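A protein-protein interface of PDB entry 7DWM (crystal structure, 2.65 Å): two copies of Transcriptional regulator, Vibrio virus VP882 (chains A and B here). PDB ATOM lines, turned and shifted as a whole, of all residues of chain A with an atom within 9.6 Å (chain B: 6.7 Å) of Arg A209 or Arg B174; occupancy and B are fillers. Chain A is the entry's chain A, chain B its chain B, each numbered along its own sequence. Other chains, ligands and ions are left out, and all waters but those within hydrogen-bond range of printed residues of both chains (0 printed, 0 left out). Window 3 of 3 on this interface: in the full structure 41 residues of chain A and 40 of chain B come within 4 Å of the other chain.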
ATOM      1  N   LEU A 172       2.908 -14.556  -4.212  1.00  0.00           N
ATOM      2  CA  LEU A 172       2.374 -13.318  -3.652  1.00  0.00           C
ATOM      3  C   LEU A 172       1.718 -12.471  -4.735  1.00  0.00           C
ATOM      4  O   LEU A 172       0.595 -11.983  -4.566  1.00  0.00           O
ATOM      5  CB  LEU A 172       3.490 -12.531  -2.963  1.00  0.00           C
ATOM      6  CG  LEU A 172       3.736 -12.709  -1.464  1.00  0.00           C
ATOM      7  CD1 LEU A 172       4.488 -11.500  -0.942  1.00  0.00           C
ATOM      8  CD2 LEU A 172       2.437 -12.911  -0.694  1.00  0.00           C
ATOM      9  N   LEU A 173       2.416 -12.282  -5.858  1.00  0.00           N
ATOM     10  CA  LEU A 173       1.878 -11.534  -6.989  1.00  0.00           C
ATOM     11  C   LEU A 173       0.663 -12.199  -7.624  1.00  0.00           C
ATOM     12  O   LEU A 173       0.033 -11.590  -8.495  1.00  0.00           O
ATOM     13  CB  LEU A 173       2.968 -11.343  -8.046  1.00  0.00           C
ATOM     14  CG  LEU A 173       4.180 -10.516  -7.624  1.00  0.00           C
ATOM     15  CD1 LEU A 173       5.260 -10.554  -8.694  1.00  0.00           C
ATOM     16  CD2 LEU A 173       3.767  -9.086  -7.327  1.00  0.00           C
ATOM     17  N   ILE A 196       8.933 -13.153   3.209  1.00  0.00           N
ATOM     18  CA  ILE A 196       8.286 -11.947   2.699  1.00  0.00           C
ATOM     19  C   ILE A 196       8.976 -10.702   3.236  1.00  0.00           C
ATOM     20  O   ILE A 196       9.133  -9.706   2.522  1.00  0.00           O
ATOM     21  CB  ILE A 196       6.785 -11.950   3.040  1.00  0.00           C
ATOM     22  CG1 ILE A 196       6.076 -13.096   2.320  1.00  0.00           C
ATOM     23  CG2 ILE A 196       6.144 -10.623   2.655  1.00  0.00           C
ATOM     24  CD1 ILE A 196       4.641 -13.273   2.741  1.00  0.00           C
ATOM     25  N   ARG A 200      10.554  -7.907   0.813  1.00  0.00           N
ATOM     26  CA  ARG A 200      10.159  -6.516   1.001  1.00  0.00           C
ATOM     27  C   ARG A 200      11.371  -5.612   1.189  1.00  0.00           C
ATOM     28  O   ARG A 200      11.489  -4.566   0.541  1.00  0.00           O
ATOM     29  CB  ARG A 200       9.219  -6.418   2.202  1.00  0.00           C
ATOM     30  CG  ARG A 200       8.257  -5.259   2.152  1.00  0.00           C
ATOM     31  CD  ARG A 200       7.775  -4.916   3.547  1.00  0.00           C
ATOM     32  NE  ARG A 200       8.783  -4.183   4.306  1.00  0.00           N
ATOM     33  CZ  ARG A 200       9.185  -4.514   5.528  1.00  0.00           C
ATOM     34  NH1 ARG A 200       8.664  -5.570   6.136  1.00  0.00           N
ATOM     35  NH2 ARG A 200      10.109  -3.787   6.143  1.00  0.00           N
ATOM     36  N   PHE A 203      13.351  -5.071  -1.896  1.00  0.00           N
ATOM     37  CA  PHE A 203      12.709  -4.099  -2.775  1.00  0.00           C
ATOM     38  C   PHE A 203      12.778  -2.680  -2.227  1.00  0.00           C
ATOM     39  O   PHE A 203      12.593  -1.724  -2.990  1.00  0.00           O
ATOM     40  CB  PHE A 203      11.245  -4.473  -3.010  1.00  0.00           C
ATOM     41  CG  PHE A 203      11.039  -5.421  -4.152  1.00  0.00           C
ATOM     42  CD1 PHE A 203      10.595  -4.962  -5.380  1.00  0.00           C
ATOM     43  CD2 PHE A 203      11.290  -6.774  -3.996  1.00  0.00           C
ATOM     44  CE1 PHE A 203      10.403  -5.837  -6.434  1.00  0.00           C
ATOM     45  CE2 PHE A 203      11.100  -7.653  -5.045  1.00  0.00           C
ATOM     46  CZ  PHE A 203      10.656  -7.185  -6.265  1.00  0.00           C
ATOM     47  N   ALA A 205      10.597  -1.742   0.042  1.00  0.00           N
ATOM     48  CA  ALA A 205       9.207  -1.419   0.316  1.00  0.00           C
ATOM     49  C   ALA A 205       8.961  -1.322   1.816  1.00  0.00           C
ATOM     50  O   ALA A 205       9.644  -1.958   2.625  1.00  0.00           O
ATOM     51  CB  ALA A 205       8.282  -2.468  -0.301  1.00  0.00           C
ATOM     52  N   GLY A 206       7.959  -0.528   2.184  1.00  0.00           N
ATOM     53  CA  GLY A 206       7.662  -0.287   3.582  1.00  0.00           C
ATOM     54  C   GLY A 206       6.666  -1.272   4.155  1.00  0.00           C
ATOM     55  O   GLY A 206       6.668  -1.534   5.362  1.00  0.00           O
ATOM     56  N   ASN A 207       5.811  -1.829   3.300  1.00  0.00           N
ATOM     57  CA  ASN A 207       4.860  -2.848   3.721  1.00  0.00           C
ATOM     58  C   ASN A 207       4.556  -3.762   2.539  1.00  0.00           C
ATOM     59  O   ASN A 207       5.069  -3.573   1.431  1.00  0.00           O
ATOM     60  CB  ASN A 207       3.587  -2.210   4.289  1.00  0.00           C
ATOM     61  CG  ASN A 207       2.989  -1.164   3.363  1.00  0.00           C
ATOM     62  OD1 ASN A 207       3.190  -1.197   2.150  1.00  0.00           O
ATOM     63  ND2 ASN A 207       2.255  -0.219   3.939  1.00  0.00           N
ATOM     64  N   LYS A 208       3.711  -4.765   2.794  1.00  0.00           N
ATOM     65  CA  LYS A 208       3.352  -5.732   1.760  1.00  0.00           C
ATOM     66  C   LYS A 208       2.714  -5.054   0.554  1.00  0.00           C
ATOM     67  O   LYS A 208       2.951  -5.455  -0.590  1.00  0.00           O
ATOM     68  CB  LYS A 208       2.421  -6.796   2.336  1.00  0.00           C
ATOM     69  CG  LYS A 208       3.147  -7.921   3.046  1.00  0.00           C
ATOM     70  CD  LYS A 208       2.179  -8.770   3.847  1.00  0.00           C
ATOM     71  CE  LYS A 208       2.907  -9.585   4.899  1.00  0.00           C
ATOM     72  NZ  LYS A 208       2.020 -10.621   5.496  1.00  0.00           N
ATOM     73  N   ARG A 209       1.881  -4.037   0.791  1.00  0.00           N
ATOM     74  CA  ARG A 209       1.173  -3.403  -0.316  1.00  0.00           C
ATOM     75  C   ARG A 209       2.136  -2.606  -1.188  1.00  0.00           C
ATOM     76  O   ARG A 209       2.046  -2.639  -2.425  1.00  0.00           O
ATOM     77  CB  ARG A 209       0.064  -2.506   0.239  1.00  0.00           C
ATOM     78  CG  ARG A 209      -0.608  -1.615  -0.783  1.00  0.00           C
ATOM     79  CD  ARG A 209      -1.211  -0.385  -0.131  1.00  0.00           C
ATOM     80  NE  ARG A 209      -2.306   0.165  -0.922  1.00  0.00           N
ATOM     81  CZ  ARG A 209      -3.484   0.517  -0.419  1.00  0.00           C
ATOM     82  NH1 ARG A 209      -4.427   1.009  -1.213  1.00  0.00           N
ATOM     83  NH2 ARG A 209      -3.719   0.383   0.879  1.00  0.00           N
ATOM     84  N   GLU A 210       3.091  -1.917  -0.559  1.00  0.00           N
ATOM     85  CA  GLU A 210       4.144  -1.259  -1.323  1.00  0.00           C
ATOM     86  C   GLU A 210       4.999  -2.278  -2.063  1.00  0.00           C
ATOM     87  O   GLU A 210       5.473  -2.008  -3.172  1.00  0.00           O
ATOM     88  CB  GLU A 210       5.008  -0.397  -0.405  1.00  0.00           C
ATOM     89  CG  GLU A 210       5.669   0.773  -1.114  1.00  0.00           C
ATOM     90  CD  GLU A 210       6.470   1.644  -0.172  1.00  0.00           C
ATOM     91  OE1 GLU A 210       6.567   1.288   1.020  1.00  0.00           O
ATOM     92  OE2 GLU A 210       7.002   2.683  -0.618  1.00  0.00           O
ATOM     93  N   LEU A 211       5.210  -3.454  -1.466  1.00  0.00           N
ATOM     94  CA  LEU A 211       5.948  -4.513  -2.148  1.00  0.00           C
ATOM     95  C   LEU A 211       5.223  -4.964  -3.408  1.00  0.00           C
ATOM     96  O   LEU A 211       5.838  -5.124  -4.467  1.00  0.00           O
ATOM     97  CB  LEU A 211       6.169  -5.699  -1.207  1.00  0.00           C
ATOM     98  CG  LEU A 211       6.636  -6.994  -1.881  1.00  0.00           C
ATOM     99  CD1 LEU A 211       7.977  -6.796  -2.577  1.00  0.00           C
ATOM    100  CD2 LEU A 211       6.712  -8.144  -0.884  1.00  0.00           C
ATOM    101  N   ILE A 212       3.912  -5.195  -3.304  1.00  0.00           N
ATOM    102  CA  ILE A 212       3.125  -5.582  -4.472  1.00  0.00           C
ATOM    103  C   ILE A 212       3.224  -4.514  -5.554  1.00  0.00           C
ATOM    104  O   ILE A 212       3.447  -4.817  -6.733  1.00  0.00           O
ATOM    105  CB  ILE A 212       1.662  -5.849  -4.075  1.00  0.00           C
ATOM    106  CG1 ILE A 212       1.563  -7.134  -3.248  1.00  0.00           C
ATOM    107  CG2 ILE A 212       0.778  -5.932  -5.315  1.00  0.00           C
ATOM    108  CD1 ILE A 212       1.649  -8.398  -4.074  1.00  0.00           C
ATOM    109  N   ASP A 213       3.076  -3.245  -5.166  1.00  0.00           N
ATOM    110  CA  ASP A 213       3.117  -2.167  -6.152  1.00  0.00           C
ATOM    111  C   ASP A 213       4.484  -2.089  -6.827  1.00  0.00           C
ATOM    112  O   ASP A 213       4.582  -2.013  -8.061  1.00  0.00           O
ATOM    113  CB  ASP A 213       2.765  -0.839  -5.485  1.00  0.00           C
ATOM    114  CG  ASP A 213       1.278  -0.692  -5.229  1.00  0.00           C
ATOM    115  OD1 ASP A 213       0.479  -1.264  -6.002  1.00  0.00           O
ATOM    116  OD2 ASP A 213       0.913  -0.007  -4.252  1.00  0.00           O
ATOM    117  N   MET A 214       5.555  -2.112  -6.031  1.00  0.00           N
ATOM    118  CA  MET A 214       6.907  -2.042  -6.575  1.00  0.00           C
ATOM    119  C   MET A 214       7.187  -3.213  -7.511  1.00  0.00           C
ATOM    120  O   MET A 214       7.715  -3.027  -8.614  1.00  0.00           O
ATOM    121  CB  MET A 214       7.924  -2.012  -5.434  1.00  0.00           C
ATOM    122  CG  MET A 214       8.167  -0.634  -4.846  1.00  0.00           C
ATOM    123  SD  MET A 214       9.333  -0.705  -3.474  1.00  0.00           S
ATOM    124  CE  MET A 214       9.004   0.856  -2.661  1.00  0.00           C
ATOM    125  N   ALA A 215       6.848  -4.431  -7.083  1.00  0.00           N
ATOM    126  CA  ALA A 215       7.120  -5.605  -7.906  1.00  0.00           C
ATOM    127  C   ALA A 215       6.322  -5.576  -9.202  1.00  0.00           C
ATOM    128  O   ALA A 215       6.844  -5.925 -10.266  1.00  0.00           O
ATOM    129  CB  ALA A 215       6.818  -6.879  -7.118  1.00  0.00           C
ATOM    130  N   MET A 216       5.049  -5.171  -9.138  1.00  0.00           N
ATOM    131  CA  MET A 216       4.249  -5.099 -10.356  1.00  0.00           C
ATOM    132  C   MET A 216       4.788  -4.039 -11.308  1.00  0.00           C
ATOM    133  O   MET A 216       4.759  -4.224 -12.531  1.00  0.00           O
ATOM    134  CB  MET A 216       2.785  -4.830 -10.017  1.00  0.00           C
ATOM    135  CG  MET A 216       2.081  -6.008  -9.363  1.00  0.00           C
ATOM    136  SD  MET A 216       2.001  -7.475 -10.413  1.00  0.00           S
ATOM    137  CE  MET A 216       0.814  -8.465  -9.504  1.00  0.00           C
ATOM    138  N   SER A 217       5.301  -2.930 -10.772  1.00  0.00           N
ATOM    139  CA  SER A 217       5.801  -1.873 -11.642  1.00  0.00           C
ATOM    140  C   SER A 217       7.193  -2.169 -12.186  1.00  0.00           C
ATOM    141  O   SER A 217       7.607  -1.530 -13.162  1.00  0.00           O
ATOM    142  CB  SER A 217       5.818  -0.537 -10.898  1.00  0.00           C
ATOM    143  OG  SER A 217       7.113  -0.247 -10.402  1.00  0.00           O
ATOM    144  N   LEU B 169     -13.105  -3.178  -8.007  1.00  0.00           N
ATOM    145  CA  LEU B 169     -12.410  -3.574  -6.785  1.00  0.00           C
ATOM    146  C   LEU B 169     -10.946  -3.153  -6.820  1.00  0.00           C
ATOM    147  O   LEU B 169     -10.393  -2.722  -5.798  1.00  0.00           O
ATOM    148  CB  LEU B 169     -12.522  -5.082  -6.574  1.00  0.00           C
ATOM    149  CG  LEU B 169     -11.872  -5.601  -5.292  1.00  0.00           C
ATOM    150  CD1 LEU B 169     -12.542  -4.990  -4.072  1.00  0.00           C
ATOM    151  CD2 LEU B 169     -11.922  -7.124  -5.237  1.00  0.00           C
ATOM    152  N   PHE B 170     -10.297  -3.294  -7.981  1.00  0.00           N
ATOM    153  CA  PHE B 170      -8.934  -2.803  -8.148  1.00  0.00           C
ATOM    154  C   PHE B 170      -8.821  -1.352  -7.715  1.00  0.00           C
ATOM    155  O   PHE B 170      -7.873  -0.970  -7.020  1.00  0.00           O
ATOM    156  CB  PHE B 170      -8.502  -2.961  -9.606  1.00  0.00           C
ATOM    157  CG  PHE B 170      -7.118  -2.448  -9.896  1.00  0.00           C
ATOM    158  CD1 PHE B 170      -6.011  -3.252  -9.681  1.00  0.00           C
ATOM    159  CD2 PHE B 170      -6.924  -1.167 -10.393  1.00  0.00           C
ATOM    160  CE1 PHE B 170      -4.734  -2.789  -9.951  1.00  0.00           C
ATOM    161  CE2 PHE B 170      -5.649  -0.697 -10.661  1.00  0.00           C
ATOM    162  CZ  PHE B 170      -4.554  -1.510 -10.439  1.00  0.00           C
ATOM    163  N   PHE B 171      -9.783  -0.527  -8.117  1.00  0.00           N
ATOM    164  CA  PHE B 171      -9.696   0.884  -7.760  1.00  0.00           C
ATOM    165  C   PHE B 171     -10.195   1.159  -6.344  1.00  0.00           C
ATOM    166  O   PHE B 171      -9.751   2.126  -5.716  1.00  0.00           O
ATOM    167  CB  PHE B 171     -10.469   1.725  -8.767  1.00  0.00           C
ATOM    168  CG  PHE B 171      -9.750   1.925 -10.064  1.00  0.00           C
ATOM    169  CD1 PHE B 171      -8.553   2.621 -10.105  1.00  0.00           C
ATOM    170  CD2 PHE B 171     -10.269   1.420 -11.242  1.00  0.00           C
ATOM    171  CE1 PHE B 171      -7.885   2.807 -11.302  1.00  0.00           C
ATOM    172  CE2 PHE B 171      -9.607   1.605 -12.442  1.00  0.00           C
ATOM    173  CZ  PHE B 171      -8.414   2.300 -12.472  1.00  0.00           C
ATOM    174  N   LEU B 172     -11.100   0.328  -5.824  1.00  0.00           N
ATOM    175  CA  LEU B 172     -11.531   0.456  -4.434  1.00  0.00           C
ATOM    176  C   LEU B 172     -10.365   0.233  -3.483  1.00  0.00           C
ATOM    177  O   LEU B 172     -10.159   1.002  -2.537  1.00  0.00           O
ATOM    178  CB  LEU B 172     -12.650  -0.542  -4.139  1.00  0.00           C
ATOM    179  CG  LEU B 172     -14.110  -0.112  -4.261  1.00  0.00           C
ATOM    180  CD1 LEU B 172     -15.002  -1.204  -3.697  1.00  0.00           C
ATOM    181  CD2 LEU B 172     -14.355   1.209  -3.546  1.00  0.00           C
ATOM    182  N   LEU B 173      -9.599  -0.835  -3.713  1.00  0.00           N
ATOM    183  CA  LEU B 173      -8.429  -1.118  -2.892  1.00  0.00           C
ATOM    184  C   LEU B 173      -7.348  -0.050  -3.009  1.00  0.00           C
ATOM    185  O   LEU B 173      -6.381  -0.090  -2.241  1.00  0.00           O
ATOM    186  CB  LEU B 173      -7.854  -2.490  -3.255  1.00  0.00           C
ATOM    187  CG  LEU B 173      -8.838  -3.656  -3.147  1.00  0.00           C
ATOM    188  CD1 LEU B 173      -8.219  -4.948  -3.660  1.00  0.00           C
ATOM    189  CD2 LEU B 173      -9.327  -3.818  -1.712  1.00  0.00           C
ATOM    190  N   ARG B 174      -7.484   0.900  -3.936  1.00  0.00           N
ATOM    191  CA  ARG B 174      -6.471   1.925  -4.162  1.00  0.00           C
ATOM    192  C   ARG B 174      -6.989   3.320  -3.821  1.00  0.00           C
ATOM    193  O   ARG B 174      -6.508   4.316  -4.365  1.00  0.00           O
ATOM    194  CB  ARG B 174      -5.970   1.878  -5.605  1.00  0.00           C
ATOM    195  CG  ARG B 174      -4.735   1.016  -5.795  1.00  0.00           C
ATOM    196  CD  ARG B 174      -4.840   0.138  -7.032  1.00  0.00           C
ATOM    197  NE  ARG B 174      -3.875  -0.958  -7.004  1.00  0.00           N
ATOM    198  CZ  ARG B 174      -4.194  -2.228  -6.772  1.00  0.00           C
ATOM    199  NH1 ARG B 174      -5.459  -2.566  -6.559  1.00  0.00           N
ATOM    200  NH2 ARG B 174      -3.252  -3.162  -6.766  1.00  0.00           N
ATOM    201  N   GLY B 175      -7.969   3.407  -2.925  1.00  0.00           N
ATOM    202  CA  GLY B 175      -8.396   4.679  -2.380  1.00  0.00           C
ATOM    203  C   GLY B 175      -9.355   5.479  -3.231  1.00  0.00           C
ATOM    204  O   GLY B 175      -9.678   6.614  -2.864  1.00  0.00           O
ATOM    205  N   ARG B 176      -9.818   4.939  -4.354  1.00  0.00           N
ATOM    206  CA  ARG B 176     -10.785   5.655  -5.171  1.00  0.00           C
ATOM    207  C   ARG B 176     -12.199   5.409  -4.656  1.00  0.00           C
ATOM    208  O   ARG B 176     -12.493   4.372  -4.054  1.00  0.00           O
ATOM    209  CB  ARG B 176     -10.679   5.231  -6.638  1.00  0.00           C
ATOM    210  CG  ARG B 176      -9.269   4.921  -7.134  1.00  0.00           C
ATOM    211  CD  ARG B 176      -8.285   6.045  -6.839  1.00  0.00           C
ATOM    212  NE  ARG B 176      -8.794   7.346  -7.255  1.00  0.00           N
ATOM    213  CZ  ARG B 176      -8.605   7.870  -8.459  1.00  0.00           C
ATOM    214  NH1 ARG B 176      -7.914   7.203  -9.374  1.00  0.00           N
ATOM    215  NH2 ARG B 176      -9.106   9.062  -8.749  1.00  0.00           N
ATOM    216  N   ILE B 212     -13.217  -3.707   1.688  1.00  0.00           N
ATOM    217  CA  ILE B 212     -11.824  -3.355   1.433  1.00  0.00           C
ATOM    218  C   ILE B 212     -10.894  -4.220   2.280  1.00  0.00           C
ATOM    219  O   ILE B 212      -9.932  -4.803   1.770  1.00  0.00           O
ATOM    220  CB  ILE B 212     -11.592  -1.853   1.684  1.00  0.00           C
ATOM    221  CG1 ILE B 212     -12.241  -1.018   0.576  1.00  0.00           C
ATOM    222  CG2 ILE B 212     -10.105  -1.552   1.788  1.00  0.00           C
ATOM    223  CD1 ILE B 212     -12.036   0.479   0.732  1.00  0.00           C
ATOM    224  N   MET B 216      -8.434  -7.067   0.791  1.00  0.00           N
ATOM    225  CA  MET B 216      -7.012  -6.817   0.988  1.00  0.00           C
ATOM    226  C   MET B 216      -6.342  -7.981   1.706  1.00  0.00           C
ATOM    227  O   MET B 216      -5.188  -8.317   1.418  1.00  0.00           O
ATOM    228  CB  MET B 216      -6.824  -5.521   1.778  1.00  0.00           C
ATOM    229  CG  MET B 216      -5.516  -4.814   1.510  1.00  0.00           C
ATOM    230  SD  MET B 216      -5.547  -3.918  -0.050  1.00  0.00           S
ATOM    231  CE  MET B 216      -6.581  -2.522   0.387  1.00  0.00           C
ATOM    232  N   TYR B 220      -6.400  -9.948  -2.824  1.00  0.00           N
ATOM    233  CA  TYR B 220      -6.981  -9.293  -3.989  1.00  0.00           C
ATOM    234  C   TYR B 220      -6.273  -8.002  -4.367  1.00  0.00           C
ATOM    235  O   TYR B 220      -6.575  -7.439  -5.425  1.00  0.00           O
ATOM    236  CB  TYR B 220      -8.470  -9.017  -3.757  1.00  0.00           C
ATOM    237  CG  TYR B 220      -9.330 -10.229  -3.997  1.00  0.00           C
ATOM    238  CD1 TYR B 220      -9.865 -10.483  -5.253  1.00  0.00           C
ATOM    239  CD2 TYR B 220      -9.584 -11.131  -2.978  1.00  0.00           C
ATOM    240  CE1 TYR B 220     -10.646 -11.606  -5.482  1.00  0.00           C
ATOM    241  CE2 TYR B 220     -10.359 -12.252  -3.194  1.00  0.00           C
ATOM    242  CZ  TYR B 220     -10.889 -12.485  -4.445  1.00  0.00           C
ATOM    243  OH  TYR B 220     -11.662 -13.605  -4.652  1.00  0.00           O
ATOM    244  N   TYR B 221      -5.350  -7.512  -3.539  1.00  0.00           N
ATOM    245  CA  TYR B 221      -4.560  -6.358  -3.947  1.00  0.00           C
ATOM    246  C   TYR B 221      -3.628  -6.674  -5.108  1.00  0.00           C
ATOM    247  O   TYR B 221      -3.236  -5.757  -5.837  1.00  0.00           O
ATOM    248  CB  TYR B 221      -3.738  -5.809  -2.783  1.00  0.00           C
ATOM    249  CG  TYR B 221      -3.155  -4.451  -3.090  1.00  0.00           C
ATOM    250  CD1 TYR B 221      -1.816  -4.307  -3.428  1.00  0.00           C
ATOM    251  CD2 TYR B 221      -3.954  -3.316  -3.075  1.00  0.00           C
ATOM    252  CE1 TYR B 221      -1.286  -3.067  -3.728  1.00  0.00           C
ATOM    253  CE2 TYR B 221      -3.433  -2.075  -3.370  1.00  0.00           C
ATOM    254  CZ  TYR B 221      -2.102  -1.956  -3.696  1.00  0.00           C
ATOM    255  OH  TYR B 221      -1.582  -0.720  -3.988  1.00  0.00           O
ATOM    256  N   SER B 222      -3.254  -7.938  -5.291  1.00  0.00           N
ATOM    257  CA  SER B 222      -2.321  -8.303  -6.344  1.00  0.00           C
ATOM    258  C   SER B 222      -3.002  -8.706  -7.645  1.00  0.00           C
ATOM    259  O   SER B 222      -2.304  -9.005  -8.619  1.00  0.00           O
ATOM    260  CB  SER B 222      -1.426  -9.451  -5.869  1.00  0.00           C
ATOM    261  OG  SER B 222      -2.087 -10.693  -6.012  1.00  0.00           O
ATOM    262  N   MET B 223      -4.330  -8.724  -7.701  1.00  0.00           N
ATOM    263  CA  MET B 223      -4.994  -9.005  -8.963  1.00  0.00           C
ATOM    264  C   MET B 223      -4.976  -7.749  -9.828  1.00  0.00           C
ATOM    265  O   MET B 223      -5.229  -6.644  -9.342  1.00  0.00           O
ATOM    266  CB  MET B 223      -6.429  -9.493  -8.741  1.00  0.00           C
ATOM    267  CG  MET B 223      -7.396  -8.451  -8.227  1.00  0.00           C
ATOM    268  SD  MET B 223      -9.037  -8.603  -8.940  1.00  0.00           S
ATOM    269  CE  MET B 223      -9.006  -7.199 -10.042  1.00  0.00           C
ATOM    270  N   VAL B 224      -4.637  -7.926 -11.092  1.00  0.00           N
ATOM    271  CA  VAL B 224      -4.742  -6.837 -12.081  1.00  0.00           C
ATOM    272  C   VAL B 224      -5.914  -7.206 -13.003  1.00  0.00           C
ATOM    273  O   VAL B 224      -6.014  -8.296 -13.496  1.00  0.00           O
ATOM    274  CB  VAL B 224      -3.432  -6.664 -12.883  1.00  0.00           C
ATOM    275  CG1 VAL B 224      -2.232  -6.729 -11.931  1.00  0.00           C
ATOM    276  CG2 VAL B 224      -3.264  -7.670 -14.010  1.00  0.00           C
ATOM    277  N   PRO B 225      -6.880  -6.254 -13.159  1.00  0.00           N
ATOM    278  CA  PRO B 225      -8.028  -6.576 -14.031  1.00  0.00           C
ATOM    279  C   PRO B 225      -7.612  -6.615 -15.487  1.00  0.00           C
ATOM    280  O   PRO B 225      -6.857  -5.763 -15.957  1.00  0.00           O
ATOM    281  CB  PRO B 225      -8.997  -5.408 -13.757  1.00  0.00           C
ATOM    282  CG  PRO B 225      -8.409  -4.632 -12.621  1.00  0.00           C
ATOM    283  CD  PRO B 225      -6.946  -4.916 -12.610  1.00  0.00           C
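The side-chain amide oxygen (OD1) of Asn A207 sits close to the backbone NH (N) of Arg A209, 3.4 Å away. O of Phe B170 is in hydrogen-bond range of NH1 of Arg B174 (2.9 Å). The guanidinium group (NH2) of Arg B174 sits at hydrogen-bond distance from the backbone carbonyl oxygen (O) of Tyr B221.
Among the printed residues, pairs that only touch across the chains: Met A216 with Ser B222 (3.3 Å), Ile A212 with Tyr B221 (3.6 Å), Arg A209 with Arg B174 (3.7 Å) and Ile A212 with Ser B222 (3.7 Å).
Of the 18 printed residues of chain A, 6 touch a printed residue of chain B. Hydrophobic or aromatic side chains of chain A that line the printed part of chain B: Ile A212 and Met A216.
Of chain B, only Leu B173 (2.5 Å), Arg B174 (3.7 Å) and Tyr B221 (3.3 Å) come within 4 Å of Arg A209. Arg B174 touches just one residue of chain A: Arg A209 (3.7 Å). Of chain A, only Arg A209 (2.5 Å) comes within 4 Å of Leu B173. Printed residues of chain A within 4 Å of Ser B222: Leu A172 (3.3 Å), Leu A173 (3.4 Å), Ile A212 (3.7 Å) and Met A216 (3.3 Å). Of the printed residues of chain B, Ile A212 touches Tyr B221 (3.6 Å) and Ser B222 (3.7 Å). Of the printed residues of chain B, Asp A213 touches Tyr B221. Of the printed residues of chain A, Tyr B221 touches Arg A209 (3.3 Å), Ile A212 (3.6 Å) and Asp A213 (2.6 Å). Of the printed residues of chain B, Leu A172 touches Ser B222 (3.3 Å). Tyr B220 touches none of the printed residues of chain A. Val B224 touches none of the printed residues of chain A.
4 positions are printed for both chains.
The backbone carbonyl oxygen (O) of Leu A172 lies within hydrogen-bond range of the side-chain hydroxyl (OG) of Ser B222 (3.3 Å). O of Leu A173 is in hydrogen-bond range of OG of Ser B222, 3.4 Å away. The guanidinium group (NH1) of Arg A209 sits at hydrogen-bond distance from the backbone carbonyl oxygen (O) of Leu B173 (2.5 Å). OH of Tyr B221 sits at hydrogen-bond distance from NE of Arg A209, at 3.3 Å. The side-chain carboxylate (OD2) of Asp A213 sits at hydrogen-bond distance from the side-chain hydroxyl (OH) of Tyr B221 (2.6 Å).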
